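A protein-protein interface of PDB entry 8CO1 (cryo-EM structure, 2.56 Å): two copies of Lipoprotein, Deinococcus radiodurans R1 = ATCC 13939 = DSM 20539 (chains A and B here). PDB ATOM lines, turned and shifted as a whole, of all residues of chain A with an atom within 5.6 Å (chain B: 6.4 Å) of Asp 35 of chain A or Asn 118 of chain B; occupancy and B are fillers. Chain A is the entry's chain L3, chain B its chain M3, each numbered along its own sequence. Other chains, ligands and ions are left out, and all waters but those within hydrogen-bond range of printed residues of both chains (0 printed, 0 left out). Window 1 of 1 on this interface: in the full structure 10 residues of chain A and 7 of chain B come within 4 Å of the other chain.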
ATOM      1  N   GLY A  33      -4.653  30.899   8.982  1.00  0.00           N
ATOM      2  CA  GLY A  33      -5.030  29.798   9.849  1.00  0.00           C
ATOM      3  C   GLY A  33      -4.362  29.931  11.203  1.00  0.00           C
ATOM      4  O   GLY A  33      -3.304  30.548  11.332  1.00  0.00           O
ATOM      5  N   VAL A  34      -4.990  29.341  12.217  1.00  0.00           N
ATOM      6  CA  VAL A  34      -4.583  29.526  13.604  1.00  0.00           C
ATOM      7  C   VAL A  34      -4.448  28.174  14.292  1.00  0.00           C
ATOM      8  O   VAL A  34      -5.317  27.304  14.160  1.00  0.00           O
ATOM      9  CB  VAL A  34      -5.576  30.437  14.357  1.00  0.00           C
ATOM     10  CG1 VAL A  34      -6.986  29.893  14.258  1.00  0.00           C
ATOM     11  CG2 VAL A  34      -5.167  30.591  15.811  1.00  0.00           C
ATOM     12  N   ASP A  35      -3.345  27.993  15.013  1.00  0.00           N
ATOM     13  CA  ASP A  35      -3.147  26.856  15.902  1.00  0.00           C
ATOM     14  C   ASP A  35      -3.292  27.356  17.334  1.00  0.00           C
ATOM     15  O   ASP A  35      -2.474  28.157  17.801  1.00  0.00           O
ATOM     16  CB  ASP A  35      -1.775  26.219  15.677  1.00  0.00           C
ATOM     17  CG  ASP A  35      -1.651  24.850  16.318  1.00  0.00           C
ATOM     18  OD1 ASP A  35      -1.874  24.734  17.541  1.00  0.00           O
ATOM     19  OD2 ASP A  35      -1.334  23.884  15.594  1.00  0.00           O
ATOM     20  N   VAL A  36      -4.322  26.880  18.029  1.00  0.00           N
ATOM     21  CA  VAL A  36      -4.738  27.517  19.275  1.00  0.00           C
ATOM     22  C   VAL A  36      -3.991  26.927  20.466  1.00  0.00           C
ATOM     23  O   VAL A  36      -3.387  27.655  21.261  1.00  0.00           O
ATOM     24  CB  VAL A  36      -6.262  27.402  19.445  1.00  0.00           C
ATOM     25  CG1 VAL A  36      -6.737  28.186  20.639  1.00  0.00           C
ATOM     26  CG2 VAL A  36      -6.960  27.841  18.183  1.00  0.00           C
ATOM     27  N   GLY A  37      -4.027  25.607  20.618  1.00  0.00           N
ATOM     28  CA  GLY A  37      -3.256  24.977  21.675  1.00  0.00           C
ATOM     29  C   GLY A  37      -3.727  25.329  23.073  1.00  0.00           C
ATOM     30  O   GLY A  37      -3.043  26.057  23.799  1.00  0.00           O
ATOM     31  N   THR A  76      -2.099  29.855  23.602  1.00  0.00           N
ATOM     32  CA  THR A  76      -1.173  30.505  22.674  1.00  0.00           C
ATOM     33  C   THR A  76      -1.706  30.386  21.250  1.00  0.00           C
ATOM     34  O   THR A  76      -1.458  29.393  20.564  1.00  0.00           O
ATOM     35  CB  THR A  76       0.218  29.893  22.789  1.00  0.00           C
ATOM     36  OG1 THR A  76       0.623  29.884  24.161  1.00  0.00           O
ATOM     37  CG2 THR A  76       1.218  30.701  21.983  1.00  0.00           C
ATOM     38  N   PHE A  77      -2.420  31.416  20.801  1.00  0.00           N
ATOM     39  CA  PHE A  77      -2.873  31.475  19.417  1.00  0.00           C
ATOM     40  C   PHE A  77      -1.679  31.685  18.493  1.00  0.00           C
ATOM     41  O   PHE A  77      -0.784  32.476  18.797  1.00  0.00           O
ATOM     42  CB  PHE A  77      -3.878  32.610  19.244  1.00  0.00           C
ATOM     43  CG  PHE A  77      -5.230  32.315  19.820  1.00  0.00           C
ATOM     44  CD1 PHE A  77      -5.464  32.459  21.175  1.00  0.00           C
ATOM     45  CD2 PHE A  77      -6.267  31.891  19.007  1.00  0.00           C
ATOM     46  CE1 PHE A  77      -6.705  32.191  21.710  1.00  0.00           C
ATOM     47  CE2 PHE A  77      -7.512  31.619  19.540  1.00  0.00           C
ATOM     48  CZ  PHE A  77      -7.728  31.771  20.895  1.00  0.00           C
ATOM     49  N   THR A  78      -1.660  30.975  17.364  1.00  0.00           N
ATOM     50  CA  THR A  78      -0.564  31.059  16.400  1.00  0.00           C
ATOM     51  C   THR A  78      -1.142  31.226  15.001  1.00  0.00           C
ATOM     52  O   THR A  78      -1.642  30.262  14.415  1.00  0.00           O
ATOM     53  CB  THR A  78       0.332  29.822  16.471  1.00  0.00           C
ATOM     54  OG1 THR A  78       0.903  29.720  17.781  1.00  0.00           O
ATOM     55  CG2 THR A  78       1.448  29.914  15.451  1.00  0.00           C
ATOM     56  N   PHE A  79      -1.053  32.440  14.462  1.00  0.00           N
ATOM     57  CA  PHE A  79      -1.616  32.777  13.161  1.00  0.00           C
ATOM     58  C   PHE A  79      -0.541  32.690  12.087  1.00  0.00           C
ATOM     59  O   PHE A  79       0.542  33.264  12.241  1.00  0.00           O
ATOM     60  CB  PHE A  79      -2.209  34.188  13.165  1.00  0.00           C
ATOM     61  CG  PHE A  79      -3.168  34.450  14.287  1.00  0.00           C
ATOM     62  CD1 PHE A  79      -2.716  34.919  15.506  1.00  0.00           C
ATOM     63  CD2 PHE A  79      -4.526  34.256  14.112  1.00  0.00           C
ATOM     64  CE1 PHE A  79      -3.599  35.171  16.534  1.00  0.00           C
ATOM     65  CE2 PHE A  79      -5.411  34.506  15.139  1.00  0.00           C
ATOM     66  CZ  PHE A  79      -4.946  34.965  16.351  1.00  0.00           C
ATOM     67  N   THR A  80      -0.844  31.979  11.001  1.00  0.00           N
ATOM     68  CA  THR A  80       0.004  31.944   9.819  1.00  0.00           C
ATOM     69  C   THR A  80      -0.853  32.155   8.581  1.00  0.00           C
ATOM     70  O   THR A  80      -2.004  31.720   8.525  1.00  0.00           O
ATOM     71  CB  THR A  80       0.768  30.620   9.677  1.00  0.00           C
ATOM     72  OG1 THR A  80      -0.156  29.528   9.708  1.00  0.00           O
ATOM     73  CG2 THR A  80       1.770  30.459  10.798  1.00  0.00           C
ATOM     74  N   ARG A  82      -1.811  31.579   4.675  1.00  0.00           N
ATOM     75  CA  ARG A  82      -1.726  30.543   3.665  1.00  0.00           C
ATOM     76  C   ARG A  82      -1.036  31.088   2.418  1.00  0.00           C
ATOM     77  O   ARG A  82      -1.023  32.298   2.188  1.00  0.00           O
ATOM     78  CB  ARG A  82      -3.122  30.026   3.323  1.00  0.00           C
ATOM     79  CG  ARG A  82      -3.595  28.875   4.205  1.00  0.00           C
ATOM     80  CD  ARG A  82      -3.838  29.334   5.629  1.00  0.00           C
ATOM     81  NE  ARG A  82      -4.007  28.227   6.561  1.00  0.00           N
ATOM     82  CZ  ARG A  82      -5.178  27.688   6.876  1.00  0.00           C
ATOM     83  NH1 ARG A  82      -6.291  28.154   6.330  1.00  0.00           N
ATOM     84  NH2 ARG A  82      -5.237  26.684   7.737  1.00  0.00           N
ATOM     85  N   THR B  89      -2.135  20.636   4.645  1.00  0.00           N
ATOM     86  CA  THR B  89      -2.239  21.272   5.950  1.00  0.00           C
ATOM     87  C   THR B  89      -3.414  20.668   6.703  1.00  0.00           C
ATOM     88  O   THR B  89      -4.534  20.627   6.182  1.00  0.00           O
ATOM     89  CB  THR B  89      -2.413  22.785   5.822  1.00  0.00           C
ATOM     90  OG1 THR B  89      -1.252  23.350   5.209  1.00  0.00           O
ATOM     91  CG2 THR B  89      -2.600  23.409   7.186  1.00  0.00           C
ATOM     92  N   ILE B  90      -3.158  20.204   7.922  1.00  0.00           N
ATOM     93  CA  ILE B  90      -4.182  19.568   8.744  1.00  0.00           C
ATOM     94  C   ILE B  90      -4.827  20.620   9.633  1.00  0.00           C
ATOM     95  O   ILE B  90      -4.136  21.361  10.342  1.00  0.00           O
ATOM     96  CB  ILE B  90      -3.584  18.430   9.583  1.00  0.00           C
ATOM     97  CG1 ILE B  90      -2.749  17.504   8.700  1.00  0.00           C
ATOM     98  CG2 ILE B  90      -4.688  17.658  10.280  1.00  0.00           C
ATOM     99  CD1 ILE B  90      -3.550  16.793   7.638  1.00  0.00           C
ATOM    100  N   GLU B  91      -6.155  20.686   9.596  1.00  0.00           N
ATOM    101  CA  GLU B  91      -6.909  21.701  10.318  1.00  0.00           C
ATOM    102  C   GLU B  91      -7.485  21.206  11.637  1.00  0.00           C
ATOM    103  O   GLU B  91      -7.571  21.983  12.592  1.00  0.00           O
ATOM    104  CB  GLU B  91      -8.046  22.226   9.437  1.00  0.00           C
ATOM    105  CG  GLU B  91      -7.595  23.225   8.387  1.00  0.00           C
ATOM    106  CD  GLU B  91      -8.742  23.735   7.548  1.00  0.00           C
ATOM    107  OE1 GLU B  91      -8.701  24.911   7.134  1.00  0.00           O
ATOM    108  OE2 GLU B  91      -9.685  22.959   7.294  1.00  0.00           O
ATOM    109  N   LYS B 116      -8.321  23.221  15.790  1.00  0.00           N
ATOM    110  CA  LYS B 116      -7.292  23.884  16.577  1.00  0.00           C
ATOM    111  C   LYS B 116      -5.907  23.586  16.016  1.00  0.00           C
ATOM    112  O   LYS B 116      -4.902  23.661  16.729  1.00  0.00           O
ATOM    113  CB  LYS B 116      -7.441  23.425  18.027  1.00  0.00           C
ATOM    114  CG  LYS B 116      -6.603  24.116  19.062  1.00  0.00           C
ATOM    115  CD  LYS B 116      -6.888  23.513  20.412  1.00  0.00           C
ATOM    116  CE  LYS B 116      -8.326  23.829  20.797  1.00  0.00           C
ATOM    117  NZ  LYS B 116      -8.525  25.282  21.066  1.00  0.00           N
ATOM    118  N   MET B 117      -5.837  23.264  14.728  1.00  0.00           N
ATOM    119  CA  MET B 117      -4.600  22.796  14.120  1.00  0.00           C
ATOM    120  C   MET B 117      -4.275  23.618  12.882  1.00  0.00           C
ATOM    121  O   MET B 117      -5.139  23.833  12.027  1.00  0.00           O
ATOM    122  CB  MET B 117      -4.709  21.314  13.758  1.00  0.00           C
ATOM    123  CG  MET B 117      -4.822  20.400  14.963  1.00  0.00           C
ATOM    124  SD  MET B 117      -5.036  18.673  14.526  1.00  0.00           S
ATOM    125  CE  MET B 117      -3.413  18.303  13.877  1.00  0.00           C
ATOM    126  N   ASN B 118      -3.031  24.089  12.801  1.00  0.00           N
ATOM    127  CA  ASN B 118      -2.439  24.609  11.568  1.00  0.00           C
ATOM    128  C   ASN B 118      -1.101  23.896  11.416  1.00  0.00           C
ATOM    129  O   ASN B 118      -0.057  24.423  11.805  1.00  0.00           O
ATOM    130  CB  ASN B 118      -2.273  26.118  11.611  1.00  0.00           C
ATOM    131  CG  ASN B 118      -2.431  26.758  10.250  1.00  0.00           C
ATOM    132  OD1 ASN B 118      -3.196  26.285   9.412  1.00  0.00           O
ATOM    133  ND2 ASN B 118      -1.694  27.834  10.016  1.00  0.00           N
ATOM    134  N   LEU B 119      -1.134  22.696  10.841  1.00  0.00           N
ATOM    135  CA  LEU B 119       0.040  21.841  10.750  1.00  0.00           C
ATOM    136  C   LEU B 119       0.355  21.586   9.286  1.00  0.00           C
ATOM    137  O   LEU B 119      -0.474  21.034   8.556  1.00  0.00           O
ATOM    138  CB  LEU B 119      -0.184  20.525  11.497  1.00  0.00           C
ATOM    139  CG  LEU B 119       1.034  19.628  11.724  1.00  0.00           C
ATOM    140  CD1 LEU B 119       2.205  20.418  12.275  1.00  0.00           C
ATOM    141  CD2 LEU B 119       0.670  18.499  12.661  1.00  0.00           C
ATOM    142  N   TYR B 120       1.553  21.980   8.866  1.00  0.00           N
ATOM    143  CA  TYR B 120       1.965  21.885   7.473  1.00  0.00           C
ATOM    144  C   TYR B 120       2.817  20.641   7.260  1.00  0.00           C
ATOM    145  O   TYR B 120       3.831  20.450   7.939  1.00  0.00           O
ATOM    146  CB  TYR B 120       2.750  23.131   7.065  1.00  0.00           C
ATOM    147  CG  TYR B 120       2.941  23.281   5.578  1.00  0.00           C
ATOM    148  CD1 TYR B 120       1.853  23.348   4.725  1.00  0.00           C
ATOM    149  CD2 TYR B 120       4.210  23.355   5.029  1.00  0.00           C
ATOM    150  CE1 TYR B 120       2.021  23.489   3.367  1.00  0.00           C
ATOM    151  CE2 TYR B 120       4.390  23.494   3.671  1.00  0.00           C
ATOM    152  CZ  TYR B 120       3.292  23.561   2.844  1.00  0.00           C
ATOM    153  OH  TYR B 120       3.464  23.701   1.487  1.00  0.00           O
ATOM    154  N   HIS B 153       2.602  16.416  16.220  1.00  0.00           N
ATOM    155  CA  HIS B 153       1.553  17.030  17.017  1.00  0.00           C
ATOM    156  C   HIS B 153       1.277  16.127  18.209  1.00  0.00           C
ATOM    157  O   HIS B 153       1.483  14.913  18.144  1.00  0.00           O
ATOM    158  CB  HIS B 153       0.273  17.251  16.203  1.00  0.00           C
ATOM    159  CG  HIS B 153      -0.813  17.939  16.967  1.00  0.00           C
ATOM    160  ND1 HIS B 153      -0.703  19.240  17.408  1.00  0.00           N
ATOM    161  CD2 HIS B 153      -2.029  17.507  17.375  1.00  0.00           C
ATOM    162  CE1 HIS B 153      -1.804  19.579  18.052  1.00  0.00           C
ATOM    163  NE2 HIS B 153      -2.626  18.545  18.046  1.00  0.00           N
ATOM    164  N   PHE B 183      -6.651  20.394   3.926  1.00  0.00           N
ATOM    165  CA  PHE B 183      -6.681  20.708   2.506  1.00  0.00           C
ATOM    166  C   PHE B 183      -5.267  20.620   1.953  1.00  0.00           C
ATOM    167  O   PHE B 183      -4.295  20.886   2.661  1.00  0.00           O
ATOM    168  CB  PHE B 183      -7.269  22.100   2.252  1.00  0.00           C
ATOM    169  CG  PHE B 183      -6.434  23.220   2.800  1.00  0.00           C
ATOM    170  CD1 PHE B 183      -6.327  23.424   4.162  1.00  0.00           C
ATOM    171  CD2 PHE B 183      -5.758  24.073   1.950  1.00  0.00           C
ATOM    172  CE1 PHE B 183      -5.558  24.450   4.662  1.00  0.00           C
ATOM    173  CE2 PHE B 183      -4.991  25.100   2.446  1.00  0.00           C
ATOM    174  CZ  PHE B 183      -4.891  25.289   3.803  1.00  0.00           C
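The backbone carbonyl oxygen (O) of Lys 116 of chain B lies close to the side-chain carboxylate (OD1) of Asp 35 of chain A, 3.3 Å away.
N of Asn 118 of chain B is in hydrogen-bond range of OD2 of Asp 35 of chain A (3.3 Å).
The side-chain hydroxyl of Thr 80 of chain A sits close to the side-chain amide nitrogen of Asn 118 of chain B (2.3 Å).
The guanidinium group (NH2) of Arg 82 of chain A sits at hydrogen-bond distance from the side-chain amide oxygen (OD1) of Asn 118 of chain B (2.7 Å).
The side-chain carboxylate (OE1) of Glu 91 of chain B is in salt-bridge range of the guanidinium group (NH2) of Arg 82 of chain A (3.9 Å).
O of Gly 33 of chain A is in hydrogen-bond range of ND2 of Asn 118 of chain B, at 3.4 Å.
The backbone NH of Met 117 of chain B lies within hydrogen-bond range of the backbone carbonyl oxygen of Glu 91 of chain B (3.0 Å).
N of Thr 89 of chain B lies within hydrogen-bond range of O of Phe 183 of chain B, 2.9 Å away.
O of Val 36 of chain A lies close to N of Thr 76 of chain A (3.5 Å).
N of Asp 35 of chain A is in hydrogen-bond range of O of Thr 78 of chain A.
N of Gly 33 of chain A is in hydrogen-bond range of O of Thr 80 of chain A, 2.8 Å away.
Among the printed residues, merely in contact across the chains: Val 36 of chain A with Lys 116 of chain B (3.3 Å), Gly 37 of chain A with Lys 116 of chain B (3.4 Å), Asp 35 of chain A with Met 117 of chain B (3.7 Å) and Arg 82 of chain A with Phe 183 of chain B (3.8 Å).
Of chain B, only Lys 116, Met 117 and Asn 118 come within 4 Å of Asp 35 of chain A.
Of the printed residues of chain A, Asn 118 of chain B touches Gly 33, Asp 35, Thr 80 and Arg 82.
Of the printed residues of chain B, Arg 82 of chain A touches Glu 91, Asn 118 and Phe 183.
Printed residues of chain A within 4 Å of Glu 91 of chain B: Arg 82 (3.9 Å).
Printed residues of chain B within 4 Å of Val 36 of chain A: Lys 116.
Phe 77 of chain A touches none of the printed residues of chain B.
Leu 119 of chain B touches none of the printed residues of chain A.
The nearest residue of chain B that does not touch Asp 35 of chain A is Leu 119 of chain B (4.9 Å).
Of the 11 printed residues of chain A, 6 touch a printed residue of chain B.
Hydrophobic or aromatic side chains of chain A that line the printed part of chain B: Val 36.
Along chain A the printed residues that touch a printed residue of chain B span positions 33 to 82.
Of the 10 printed residues of chain B, 5 touch a printed residue of chain A.
Hydrophobic or aromatic side chains of chain B that line the printed part of chain A: Phe 183.
Among the printed residues, Asp or Glu carboxylates within 4 Å of a Lys or Arg side-chain nitrogen of the other chain: Arg 82 of chain A with Glu 91 of chain B (3.9 Å).
No position is printed for both chains.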
